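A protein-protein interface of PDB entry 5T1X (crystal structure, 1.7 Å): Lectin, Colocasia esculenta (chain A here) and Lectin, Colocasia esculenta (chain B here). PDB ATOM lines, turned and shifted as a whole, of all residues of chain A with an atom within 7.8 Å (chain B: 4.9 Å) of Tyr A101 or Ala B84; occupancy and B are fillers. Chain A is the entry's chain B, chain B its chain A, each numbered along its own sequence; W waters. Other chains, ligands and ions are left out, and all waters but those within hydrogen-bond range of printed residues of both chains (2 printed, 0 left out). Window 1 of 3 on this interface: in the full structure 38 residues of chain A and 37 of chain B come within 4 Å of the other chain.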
ATOM      1  N   LEU A   8      -2.338  20.254  28.519  1.00  0.00           N
ATOM      2  CA  LEU A   8      -1.008  19.735  28.860  1.00  0.00           C
ATOM      3  C   LEU A   8      -0.899  19.253  30.285  1.00  0.00           C
ATOM      4  O   LEU A   8      -1.549  19.799  31.176  1.00  0.00           O
ATOM      5  CB  LEU A   8       0.055  20.848  28.688  1.00  0.00           C
ATOM      6  CG  LEU A   8       0.043  21.703  27.418  1.00  0.00           C
ATOM      7  CD1 LEU A   8       1.021  22.853  27.557  1.00  0.00           C
ATOM      8  CD2 LEU A   8       0.375  20.878  26.177  1.00  0.00           C
ATOM      9  N   LEU A   9       0.009  18.300  30.512  1.00  0.00           N
ATOM     10  CA  LEU A   9       0.381  17.826  31.835  1.00  0.00           C
ATOM     11  C   LEU A   9       1.891  17.624  31.838  1.00  0.00           C
ATOM     12  O   LEU A   9       2.385  16.704  31.194  1.00  0.00           O
ATOM     13  CB  LEU A   9      -0.382  16.546  32.253  1.00  0.00           C
ATOM     14  CG  LEU A   9      -0.326  16.236  33.758  1.00  0.00           C
ATOM     15  CD1 LEU A   9      -1.225  17.167  34.536  1.00  0.00           C
ATOM     16  CD2 LEU A   9      -0.710  14.801  34.038  1.00  0.00           C
ATOM     17  N   PHE A  10       2.625  18.540  32.483  1.00  0.00           N
ATOM     18  CA  PHE A  10       4.077  18.446  32.547  1.00  0.00           C
ATOM     19  C   PHE A  10       4.481  17.531  33.689  1.00  0.00           C
ATOM     20  O   PHE A  10       3.696  17.337  34.635  1.00  0.00           O
ATOM     21  CB  PHE A  10       4.708  19.838  32.740  1.00  0.00           C
ATOM     22  CG  PHE A  10       4.533  20.753  31.560  1.00  0.00           C
ATOM     23  CD1 PHE A  10       5.392  20.679  30.469  1.00  0.00           C
ATOM     24  CD2 PHE A  10       3.501  21.691  31.532  1.00  0.00           C
ATOM     25  CE1 PHE A  10       5.225  21.527  29.366  1.00  0.00           C
ATOM     26  CE2 PHE A  10       3.334  22.535  30.427  1.00  0.00           C
ATOM     27  CZ  PHE A  10       4.194  22.444  29.350  1.00  0.00           C
ATOM     28  N   SER A  11       5.702  16.966  33.613  1.00  0.00           N
ATOM     29  CA  SER A  11       6.272  16.155  34.693  1.00  0.00           C
ATOM     30  C   SER A  11       6.097  16.869  36.040  1.00  0.00           C
ATOM     31  O   SER A  11       6.419  18.059  36.151  1.00  0.00           O
ATOM     32  CB  SER A  11       7.764  15.923  34.447  1.00  0.00           C
ATOM     33  OG  SER A  11       7.983  15.097  33.314  1.00  0.00           O
ATOM     34  N   LEU A  60       2.815  12.352  35.940  1.00  0.00           N
ATOM     35  CA  LEU A  60       3.853  12.035  34.970  1.00  0.00           C
ATOM     36  C   LEU A  60       5.193  12.308  35.643  1.00  0.00           C
ATOM     37  O   LEU A  60       5.381  13.404  36.195  1.00  0.00           O
ATOM     38  CB  LEU A  60       3.661  12.899  33.720  1.00  0.00           C
ATOM     39  CG  LEU A  60       4.722  12.789  32.613  1.00  0.00           C
ATOM     40  CD1 LEU A  60       4.831  11.347  32.047  1.00  0.00           C
ATOM     41  CD2 LEU A  60       4.432  13.799  31.525  1.00  0.00           C
ATOM     42  N   GLY A  64       9.364   9.948  31.934  1.00  0.00           N
ATOM     43  CA  GLY A  64       8.336   9.652  30.943  1.00  0.00           C
ATOM     44  C   GLY A  64       7.327   8.589  31.293  1.00  0.00           C
ATOM     45  O   GLY A  64       6.580   8.163  30.414  1.00  0.00           O
ATOM     46  N   ASP A  87      12.736  16.465  31.510  1.00  0.00           N
ATOM     47  CA  ASP A  87      11.375  17.001  31.551  1.00  0.00           C
ATOM     48  C   ASP A  87      10.514  16.396  30.441  1.00  0.00           C
ATOM     49  O   ASP A  87      10.956  16.321  29.298  1.00  0.00           O
ATOM     50  CB  ASP A  87      11.408  18.527  31.440  1.00  0.00           C
ATOM     51  CG  ASP A  87      12.170  19.165  32.586  1.00  0.00           C
ATOM     52  OD1 ASP A  87      12.195  18.568  33.692  1.00  0.00           O
ATOM     53  OD2 ASP A  87      12.782  20.232  32.367  1.00  0.00           O
ATOM     54  N   TYR A  88       9.293  15.969  30.793  1.00  0.00           N
ATOM     55  CA  TYR A  88       8.321  15.342  29.877  1.00  0.00           C
ATOM     56  C   TYR A  88       7.012  16.109  29.856  1.00  0.00           C
ATOM     57  O   TYR A  88       6.729  16.889  30.766  1.00  0.00           O
ATOM     58  CB  TYR A  88       8.065  13.869  30.283  1.00  0.00           C
ATOM     59  CG  TYR A  88       9.249  12.971  29.981  1.00  0.00           C
ATOM     60  CD1 TYR A  88       9.251  12.141  28.867  1.00  0.00           C
ATOM     61  CD2 TYR A  88      10.405  13.019  30.759  1.00  0.00           C
ATOM     62  CE1 TYR A  88      10.358  11.343  28.559  1.00  0.00           C
ATOM     63  CE2 TYR A  88      11.531  12.250  30.441  1.00  0.00           C
ATOM     64  CZ  TYR A  88      11.495  11.404  29.347  1.00  0.00           C
ATOM     65  OH  TYR A  88      12.603  10.658  29.012  1.00  0.00           O
ATOM     66  N   VAL A  89       6.207  15.893  28.803  1.00  0.00           N
ATOM     67  CA  VAL A  89       4.897  16.519  28.711  1.00  0.00           C
ATOM     68  C   VAL A  89       3.911  15.513  28.123  1.00  0.00           C
ATOM     69  O   VAL A  89       4.247  14.792  27.189  1.00  0.00           O
ATOM     70  CB  VAL A  89       4.918  17.861  27.915  1.00  0.00           C
ATOM     71  CG1 VAL A  89       5.290  17.642  26.447  1.00  0.00           C
ATOM     72  CG2 VAL A  89       3.581  18.609  28.030  1.00  0.00           C
ATOM     73  N   LEU A  90       2.721  15.450  28.707  1.00  0.00           N
ATOM     74  CA  LEU A  90       1.605  14.670  28.183  1.00  0.00           C
ATOM     75  C   LEU A  90       0.709  15.670  27.495  1.00  0.00           C
ATOM     76  O   LEU A  90       0.298  16.647  28.134  1.00  0.00           O
ATOM     77  CB  LEU A  90       0.862  13.941  29.331  1.00  0.00           C
ATOM     78  CG  LEU A  90      -0.500  13.313  28.981  1.00  0.00           C
ATOM     79  CD1 LEU A  90      -0.355  12.081  28.110  1.00  0.00           C
ATOM     80  CD2 LEU A  90      -1.253  12.936  30.256  1.00  0.00           C
ATOM     81  N   ILE A  91       0.441  15.473  26.194  1.00  0.00           N
ATOM     82  CA  ILE A  91      -0.414  16.382  25.452  1.00  0.00           C
ATOM     83  C   ILE A  91      -1.689  15.671  25.043  1.00  0.00           C
ATOM     84  O   ILE A  91      -1.623  14.640  24.379  1.00  0.00           O
ATOM     85  CB  ILE A  91       0.285  16.982  24.191  1.00  0.00           C
ATOM     86  CG1 ILE A  91       1.677  17.602  24.522  1.00  0.00           C
ATOM     87  CG2 ILE A  91      -0.638  18.012  23.488  1.00  0.00           C
ATOM     88  CD1 ILE A  91       2.464  18.089  23.294  1.00  0.00           C
ATOM     89  N   LEU A  92      -2.845  16.259  25.383  1.00  0.00           N
ATOM     90  CA  LEU A  92      -4.116  15.798  24.841  1.00  0.00           C
ATOM     91  C   LEU A  92      -4.239  16.587  23.558  1.00  0.00           C
ATOM     92  O   LEU A  92      -4.539  17.787  23.590  1.00  0.00           O
ATOM     93  CB  LEU A  92      -5.307  16.006  25.803  1.00  0.00           C
ATOM     94  CG  LEU A  92      -6.684  15.580  25.235  1.00  0.00           C
ATOM     95  CD1 LEU A  92      -6.747  14.078  24.946  1.00  0.00           C
ATOM     96  CD2 LEU A  92      -7.820  16.025  26.145  1.00  0.00           C
ATOM     97  N   ARG A  93      -3.854  15.964  22.450  1.00  0.00           N
ATOM     98  CA  ARG A  93      -3.778  16.633  21.156  1.00  0.00           C
ATOM     99  C   ARG A  93      -5.132  17.001  20.583  1.00  0.00           C
ATOM    100  O   ARG A  93      -6.146  16.387  20.915  1.00  0.00           O
ATOM    101  CB  ARG A  93      -3.020  15.739  20.165  1.00  0.00           C
ATOM    102  CG  ARG A  93      -1.586  15.577  20.654  1.00  0.00           C
ATOM    103  CD  ARG A  93      -0.656  14.748  19.805  1.00  0.00           C
ATOM    104  NE  ARG A  93      -1.172  14.058  18.733  1.00  0.00           N
ATOM    105  CZ  ARG A  93      -0.509  13.236  17.859  1.00  0.00           C
ATOM    106  NH1 ARG A  93       0.783  13.003  17.998  1.00  0.00           N
ATOM    107  NH2 ARG A  93      -1.169  12.661  16.866  1.00  0.00           N
ATOM    108  N   ASP A  95      -6.172  16.211  17.785  1.00  0.00           N
ATOM    109  CA  ASP A  95      -6.673  15.061  17.025  1.00  0.00           C
ATOM    110  C   ASP A  95      -7.154  13.903  17.942  1.00  0.00           C
ATOM    111  O   ASP A  95      -7.501  12.849  17.429  1.00  0.00           O
ATOM    112  CB  ASP A  95      -5.634  14.570  15.989  1.00  0.00           C
ATOM    113  CG  ASP A  95      -4.295  14.106  16.538  1.00  0.00           C
ATOM    114  OD1 ASP A  95      -4.149  14.040  17.773  1.00  0.00           O
ATOM    115  OD2 ASP A  95      -3.420  13.733  15.728  1.00  0.00           O
ATOM    116  N   PHE A  97      -5.582  12.016  20.238  1.00  0.00           N
ATOM    117  CA  PHE A  97      -4.535  11.178  20.824  1.00  0.00           C
ATOM    118  C   PHE A  97      -3.971  11.846  22.075  1.00  0.00           C
ATOM    119  O   PHE A  97      -3.879  13.068  22.111  1.00  0.00           O
ATOM    120  CB  PHE A  97      -3.384  10.976  19.823  1.00  0.00           C
ATOM    121  CG  PHE A  97      -3.707  10.129  18.616  1.00  0.00           C
ATOM    122  CD1 PHE A  97      -3.582   8.746  18.665  1.00  0.00           C
ATOM    123  CD2 PHE A  97      -4.119  10.713  17.428  1.00  0.00           C
ATOM    124  CE1 PHE A  97      -3.873   7.964  17.546  1.00  0.00           C
ATOM    125  CE2 PHE A  97      -4.403   9.928  16.305  1.00  0.00           C
ATOM    126  CZ  PHE A  97      -4.274   8.563  16.373  1.00  0.00           C
ATOM    127  N   ALA A  98      -3.597  11.058  23.088  1.00  0.00           N
ATOM    128  CA  ALA A  98      -2.907  11.595  24.270  1.00  0.00           C
ATOM    129  C   ALA A  98      -1.510  11.024  24.197  1.00  0.00           C
ATOM    130  O   ALA A  98      -1.354   9.799  24.141  1.00  0.00           O
ATOM    131  CB  ALA A  98      -3.627  11.212  25.557  1.00  0.00           C
ATOM    132  N   VAL A  99      -0.495  11.891  24.056  1.00  0.00           N
ATOM    133  CA  VAL A  99       0.865  11.409  23.800  1.00  0.00           C
ATOM    134  C   VAL A  99       1.862  11.983  24.792  1.00  0.00           C
ATOM    135  O   VAL A  99       1.829  13.177  25.079  1.00  0.00           O
ATOM    136  CB  VAL A  99       1.281  11.776  22.345  1.00  0.00           C
ATOM    137  CG1 VAL A  99       2.692  11.268  22.021  1.00  0.00           C
ATOM    138  CG2 VAL A  99       0.273  11.239  21.325  1.00  0.00           C
ATOM    139  N   ILE A 100       2.778  11.137  25.278  1.00  0.00           N
ATOM    140  CA  ILE A 100       3.856  11.595  26.171  1.00  0.00           C
ATOM    141  C   ILE A 100       5.075  11.871  25.315  1.00  0.00           C
ATOM    142  O   ILE A 100       5.570  10.967  24.621  1.00  0.00           O
ATOM    143  CB  ILE A 100       4.195  10.594  27.302  1.00  0.00           C
ATOM    144  CG1 ILE A 100       2.950  10.211  28.149  1.00  0.00           C
ATOM    145  CG2 ILE A 100       5.367  11.145  28.187  1.00  0.00           C
ATOM    146  CD1 ILE A 100       3.221   9.051  29.112  1.00  0.00           C
ATOM    147  N   TYR A 101       5.580  13.101  25.395  1.00  0.00           N
ATOM    148  CA  TYR A 101       6.790  13.502  24.686  1.00  0.00           C
ATOM    149  C   TYR A 101       7.890  13.831  25.648  1.00  0.00           C
ATOM    150  O   TYR A 101       7.675  14.587  26.592  1.00  0.00           O
ATOM    151  CB  TYR A 101       6.540  14.747  23.813  1.00  0.00           C
ATOM    152  CG  TYR A 101       5.590  14.544  22.658  1.00  0.00           C
ATOM    153  CD1 TYR A 101       6.059  14.161  21.404  1.00  0.00           C
ATOM    154  CD2 TYR A 101       4.246  14.883  22.773  1.00  0.00           C
ATOM    155  CE1 TYR A 101       5.198  14.023  20.321  1.00  0.00           C
ATOM    156  CE2 TYR A 101       3.375  14.768  21.691  1.00  0.00           C
ATOM    157  CZ  TYR A 101       3.858  14.343  20.462  1.00  0.00           C
ATOM    158  OH  TYR A 101       3.010  14.190  19.387  1.00  0.00           O
ATOM    159  N   GLY A 102       9.089  13.367  25.337  1.00  0.00           N
ATOM    160  CA  GLY A 102      10.266  13.735  26.117  1.00  0.00           C
ATOM    161  C   GLY A 102      11.489  12.873  25.865  1.00  0.00           C
ATOM    162  O   GLY A 102      11.414  11.839  25.206  1.00  0.00           O
ATOM    163  N   PRO A 103      12.630  13.247  26.460  1.00  0.00           N
ATOM    164  CA  PRO A 103      12.841  14.425  27.314  1.00  0.00           C
ATOM    165  C   PRO A 103      12.929  15.732  26.523  1.00  0.00           C
ATOM    166  O   PRO A 103      12.935  15.717  25.285  1.00  0.00           O
ATOM    167  CB  PRO A 103      14.179  14.098  27.994  1.00  0.00           C
ATOM    168  CG  PRO A 103      14.937  13.342  26.920  1.00  0.00           C
ATOM    169  CD  PRO A 103      13.880  12.481  26.263  1.00  0.00           C
ATOM    170  N   ALA A 104      13.008  16.864  27.244  1.00  0.00           N
ATOM    171  CA  ALA A 104      13.236  18.167  26.618  1.00  0.00           C
ATOM    172  C   ALA A 104      14.648  18.162  26.016  1.00  0.00           C
ATOM    173  O   ALA A 104      15.588  17.796  26.722  1.00  0.00           O
ATOM    174  CB  ALA A 104      13.098  19.274  27.658  1.00  0.00           C
ATOM    175  N   ILE A 105      14.804  18.525  24.722  1.00  0.00           N
ATOM    176  CA  ILE A 105      16.120  18.518  24.056  1.00  0.00           C
ATOM    177  C   ILE A 105      16.602  19.939  23.712  1.00  0.00           C
ATOM    178  O   ILE A 105      17.780  20.130  23.386  1.00  0.00           O
ATOM    179  CB  ILE A 105      16.105  17.614  22.783  1.00  0.00           C
ATOM    180  CG1 ILE A 105      15.169  18.195  21.695  1.00  0.00           C
ATOM    181  CG2 ILE A 105      15.706  16.158  23.145  1.00  0.00           C
ATOM    182  CD1 ILE A 105      15.408  17.660  20.264  1.00  0.00           C
ATOM    183  N   TRP A 106      15.686  20.916  23.725  1.00  0.00           N
ATOM    184  CA  TRP A 106      15.988  22.310  23.383  1.00  0.00           C
ATOM    185  C   TRP A 106      15.005  23.219  24.079  1.00  0.00           C
ATOM    186  O   TRP A 106      13.825  22.875  24.186  1.00  0.00           O
ATOM    187  CB  TRP A 106      15.922  22.509  21.856  1.00  0.00           C
ATOM    188  CG  TRP A 106      16.341  23.868  21.380  1.00  0.00           C
ATOM    189  CD1 TRP A 106      17.591  24.248  20.987  1.00  0.00           C
ATOM    190  CD2 TRP A 106      15.498  25.017  21.210  1.00  0.00           C
ATOM    191  NE1 TRP A 106      17.586  25.568  20.597  1.00  0.00           N
ATOM    192  CE2 TRP A 106      16.319  26.072  20.747  1.00  0.00           C
ATOM    193  CE3 TRP A 106      14.133  25.272  21.438  1.00  0.00           C
ATOM    194  CZ2 TRP A 106      15.813  27.349  20.470  1.00  0.00           C
ATOM    195  CZ3 TRP A 106      13.636  26.537  21.165  1.00  0.00           C
ATOM    196  CH2 TRP A 106      14.469  27.555  20.672  1.00  0.00           C
ATOM    197  N   LEU B   6       3.465  22.873  18.461  1.00  0.00           N
ATOM    198  CA  LEU B   6       3.770  22.560  17.078  1.00  0.00           C
ATOM    199  C   LEU B   6       4.340  21.149  17.049  1.00  0.00           C
ATOM    200  O   LEU B   6       5.352  20.889  17.699  1.00  0.00           O
ATOM    201  CB  LEU B   6       4.773  23.589  16.503  1.00  0.00           C
ATOM    202  CG  LEU B   6       5.338  23.317  15.108  1.00  0.00           C
ATOM    203  CD1 LEU B   6       4.356  23.696  14.048  1.00  0.00           C
ATOM    204  CD2 LEU B   6       6.626  24.094  14.875  1.00  0.00           C
ATOM    205  N   LEU B   7       3.681  20.232  16.327  1.00  0.00           N
ATOM    206  CA  LEU B   7       4.170  18.852  16.219  1.00  0.00           C
ATOM    207  C   LEU B   7       5.037  18.704  14.983  1.00  0.00           C
ATOM    208  O   LEU B   7       4.844  19.436  14.003  1.00  0.00           O
ATOM    209  CB  LEU B   7       3.004  17.846  16.144  1.00  0.00           C
ATOM    210  CG  LEU B   7       1.954  17.874  17.250  1.00  0.00           C
ATOM    211  CD1 LEU B   7       0.860  16.867  16.973  1.00  0.00           C
ATOM    212  CD2 LEU B   7       2.575  17.660  18.626  1.00  0.00           C
ATOM    213  N   LEU B  55       9.079  21.715  12.359  1.00  0.00           N
ATOM    214  CA  LEU B  55       9.798  20.884  13.315  1.00  0.00           C
ATOM    215  C   LEU B  55      10.115  19.575  12.618  1.00  0.00           C
ATOM    216  O   LEU B  55       9.202  18.902  12.147  1.00  0.00           O
ATOM    217  CB  LEU B  55       8.945  20.694  14.584  1.00  0.00           C
ATOM    218  CG  LEU B  55       9.506  19.836  15.731  1.00  0.00           C
ATOM    219  CD1 LEU B  55      10.739  20.471  16.353  1.00  0.00           C
ATOM    220  CD2 LEU B  55       8.452  19.648  16.805  1.00  0.00           C
ATOM    221  N   ASN B  82       8.570  11.303  16.543  1.00  0.00           N
ATOM    222  CA  ASN B  82       7.551  12.349  16.696  1.00  0.00           C
ATOM    223  C   ASN B  82       7.934  13.279  17.824  1.00  0.00           C
ATOM    224  O   ASN B  82       8.162  12.824  18.947  1.00  0.00           O
ATOM    225  CB  ASN B  82       6.173  11.722  16.973  1.00  0.00           C
ATOM    226  CG  ASN B  82       5.686  10.779  15.898  1.00  0.00           C
ATOM    227  OD1 ASN B  82       5.718  11.081  14.711  1.00  0.00           O
ATOM    228  ND2 ASN B  82       5.200   9.618  16.301  1.00  0.00           N
ATOM    229  N   TYR B  83       7.990  14.584  17.527  1.00  0.00           N
ATOM    230  CA  TYR B  83       8.398  15.599  18.495  1.00  0.00           C
ATOM    231  C   TYR B  83       7.305  16.632  18.688  1.00  0.00           C
ATOM    232  O   TYR B  83       6.393  16.740  17.863  1.00  0.00           O
ATOM    233  CB  TYR B  83       9.699  16.280  18.017  1.00  0.00           C
ATOM    234  CG  TYR B  83      10.905  15.373  18.145  1.00  0.00           C
ATOM    235  CD1 TYR B  83      11.763  15.476  19.232  1.00  0.00           C
ATOM    236  CD2 TYR B  83      11.171  14.392  17.193  1.00  0.00           C
ATOM    237  CE1 TYR B  83      12.843  14.608  19.387  1.00  0.00           C
ATOM    238  CE2 TYR B  83      12.230  13.497  17.352  1.00  0.00           C
ATOM    239  CZ  TYR B  83      13.063  13.613  18.454  1.00  0.00           C
ATOM    240  OH  TYR B  83      14.111  12.753  18.637  1.00  0.00           O
ATOM    241  N   ALA B  84       7.416  17.401  19.766  1.00  0.00           N
ATOM    242  CA  ALA B  84       6.463  18.474  20.054  1.00  0.00           C
ATOM    243  C   ALA B  84       7.191  19.696  20.602  1.00  0.00           C
ATOM    244  O   ALA B  84       7.951  19.569  21.567  1.00  0.00           O
ATOM    245  CB  ALA B  84       5.412  17.993  21.050  1.00  0.00           C
ATOM    246  N   ALA B  85       6.976  20.866  19.981  1.00  0.00           N
ATOM    247  CA  ALA B  85       7.498  22.148  20.465  1.00  0.00           C
ATOM    248  C   ALA B  85       6.354  22.787  21.222  1.00  0.00           C
ATOM    249  O   ALA B  85       5.301  23.022  20.633  1.00  0.00           O
ATOM    250  CB  ALA B  85       7.979  23.026  19.320  1.00  0.00           C
ATOM    251  N   VAL B  86       6.510  22.957  22.538  1.00  0.00           N
ATOM    252  CA  VAL B  86       5.428  23.394  23.428  1.00  0.00           C
ATOM    253  C   VAL B  86       5.753  24.716  24.084  1.00  0.00           C
ATOM    254  O   VAL B  86       6.865  24.905  24.579  1.00  0.00           O
ATOM    255  CB  VAL B  86       5.168  22.297  24.505  1.00  0.00           C
ATOM    256  CG1 VAL B  86       4.082  22.719  25.501  1.00  0.00           C
ATOM    257  CG2 VAL B  86       4.801  20.969  23.858  1.00  0.00           C
ATOM    258  N   VAL B  94       9.801  24.964  24.393  1.00  0.00           N
ATOM    259  CA  VAL B  94      10.585  23.758  24.658  1.00  0.00           C
ATOM    260  C   VAL B  94      10.261  22.680  23.637  1.00  0.00           C
ATOM    261  O   VAL B  94       9.086  22.391  23.400  1.00  0.00           O
ATOM    262  CB  VAL B  94      10.321  23.231  26.110  1.00  0.00           C
ATOM    263  CG1 VAL B  94      11.231  22.055  26.450  1.00  0.00           C
ATOM    264  CG2 VAL B  94      10.474  24.332  27.164  1.00  0.00           C
ATOM    265  N   VAL B  95      11.303  22.026  23.106  1.00  0.00           N
ATOM    266  CA  VAL B  95      11.117  20.896  22.198  1.00  0.00           C
ATOM    267  C   VAL B  95      11.245  19.632  23.018  1.00  0.00           C
ATOM    268  O   VAL B  95      12.288  19.411  23.626  1.00  0.00           O
ATOM    269  CB  VAL B  95      12.114  20.892  21.011  1.00  0.00           C
ATOM    270  CG1 VAL B  95      11.909  19.655  20.135  1.00  0.00           C
ATOM    271  CG2 VAL B  95      12.011  22.161  20.181  1.00  0.00           C
ATOM    272  N   PHE B  96      10.195  18.791  23.014  1.00  0.00           N
ATOM    273  CA  PHE B  96      10.176  17.504  23.716  1.00  0.00           C
ATOM    274  C   PHE B  96      10.123  16.371  22.743  1.00  0.00           C
ATOM    275  O   PHE B  96       9.286  16.391  21.834  1.00  0.00           O
ATOM    276  CB  PHE B  96       8.923  17.402  24.592  1.00  0.00           C
ATOM    277  CG  PHE B  96       8.812  18.371  25.743  1.00  0.00           C
ATOM    278  CD1 PHE B  96       9.276  18.030  27.002  1.00  0.00           C
ATOM    279  CD2 PHE B  96       8.162  19.591  25.583  1.00  0.00           C
ATOM    280  CE1 PHE B  96       9.142  18.912  28.078  1.00  0.00           C
ATOM    281  CE2 PHE B  96       8.010  20.467  26.665  1.00  0.00           C
ATOM    282  CZ  PHE B  96       8.502  20.123  27.904  1.00  0.00           C
ATOM    283  N   GLY B  97      10.937  15.347  22.964  1.00  0.00           N
ATOM    284  CA  GLY B  97      10.823  14.177  22.121  1.00  0.00           C
ATOM    285  C   GLY B  97      11.959  13.189  22.188  1.00  0.00           C
ATOM    286  O   GLY B  97      13.007  13.486  22.771  1.00  0.00           O
ATOM    287  N   PRO B  98      11.788  12.023  21.525  1.00  0.00           N
ATOM    288  CA  PRO B  98      10.600  11.585  20.764  1.00  0.00           C
ATOM    289  C   PRO B  98       9.452  11.148  21.669  1.00  0.00           C
ATOM    290  O   PRO B  98       9.593  11.115  22.888  1.00  0.00           O
ATOM    291  CB  PRO B  98      11.136  10.402  19.944  1.00  0.00           C
ATOM    292  CG  PRO B  98      12.182   9.804  20.840  1.00  0.00           C
ATOM    293  CD  PRO B  98      12.843  10.987  21.515  1.00  0.00           C
ATOM    294  N   SER B  99       8.314  10.800  21.071  1.00  0.00           N
ATOM    295  CA  SER B  99       7.192  10.308  21.857  1.00  0.00           C
ATOM    296  C   SER B  99       7.558   8.952  22.430  1.00  0.00           C
ATOM    297  O   SER B  99       8.291   8.181  21.786  1.00  0.00           O
ATOM    298  CB  SER B  99       5.931  10.220  21.007  1.00  0.00           C
ATOM    299  OG  SER B  99       6.113   9.366  19.894  1.00  0.00           O
HETATM  300  O   HOH W   1       4.574  14.668  17.190  1.00  0.00           O
HETATM  301  O   HOH W   2       2.721  11.161  17.367  1.00  0.00           O
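Of the 24 printed residues of chain A, 15 touch a printed residue of chain B.
Of the 14 printed residues of chain B, 11 touch a printed residue of chain A.
Along chain B the printed residues that touch a printed residue of chain A span positions 7 to 99.
Among the printed residues, 28 pairs touch across the chains.
Among the printed residues, no Asp or Glu carboxylate lies within 4 Å of a Lys or Arg side-chain nitrogen of the other chain.
Leu A8 touches Val B86.
Phe B96 touches Asp A87.
CG1 of Val A89 touches CD2 of Phe B96, 3.6 Å away.
Ile A91 touches Ala B84.
CD1 of Ile A91 touches CG2 of Val B86 (3.8 Å).
Val A99 touches Ser B99 (CG1 to CB, 3.6 Å).
Tyr A101 touches Leu B7.
Tyr A101 touches Phe B96.
Ala A104 touches Val B94.
Ala A104 touches Val B95.
The backbone carbonyl oxygen of Val B95 lies within hydrogen-bond range of the backbone NH of Ile A105 (2.9 Å).
The backbone NH of Val B95 sits at hydrogen-bond distance from the backbone carbonyl oxygen of Trp A106, at 2.9 Å.
The backbone NH (N) of Gly B97 lies within hydrogen-bond range of the backbone carbonyl oxygen (O) of Pro A103 (3.1 Å).
The backbone NH (N) of Gly A102 sits at hydrogen-bond distance from the backbone carbonyl oxygen (O) of Pro B98 (3.4 Å).
The backbone carbonyl oxygen of Gly B97 lies close to the backbone carbonyl oxygen of Gly A102 (3.3 Å).
Of the printed residues of chain B, Phe A10 touches Val B86 and Phe B96.
Gly A64 touches none of the printed residues of chain B.
Of the printed residues of chain B, Val A89 touches Phe B96 (3.6 Å).
Asp A95 touches none of the printed residues of chain B.
Of the printed residues of chain B, Tyr A101 touches Leu B7, Asn B82, Tyr B83, Ala B84, Phe B96 and Ser B99.
Ala B84 touches just these residues of chain A: Ile A91 (3.7 Å) and Tyr A101 (3.7 Å).
Printed residues of chain A within 4 Å of Ser B99: Val A99, Ile A100 and Tyr A101.
The nearest residue of chain B that does not touch Tyr A101 is Pro B98 (4.1 Å).
The backbone NH (N) of Ser B99 sits at hydrogen-bond distance from the backbone carbonyl oxygen (O) of Asn B82 (2.9 Å).
O of Val B94 sits at hydrogen-bond distance from N of Val B86.
OG of Ser A11 sits at hydrogen-bond distance from N of Tyr A88 (3.0 Å).
The backbone carbonyl oxygen (O) of Asp A87 is in hydrogen-bond range of the backbone NH (N) of Ala A104, 3.0 Å away.
N of Ile A91 sits at hydrogen-bond distance from O of Val A99, at 2.9 Å.
OD2 of Asp A95 lies within salt-bridge range of NH2 of Arg A93, at 2.7 Å.
Water W1 bridges the side-chain hydroxyl of Tyr A101 (2.7 Å) and the backbone carbonyl oxygen of Tyr B83 (2.8 Å).
Water W2 bridges the guanidinium group of Arg A93 and the side-chain amide nitrogen of Asn B82.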
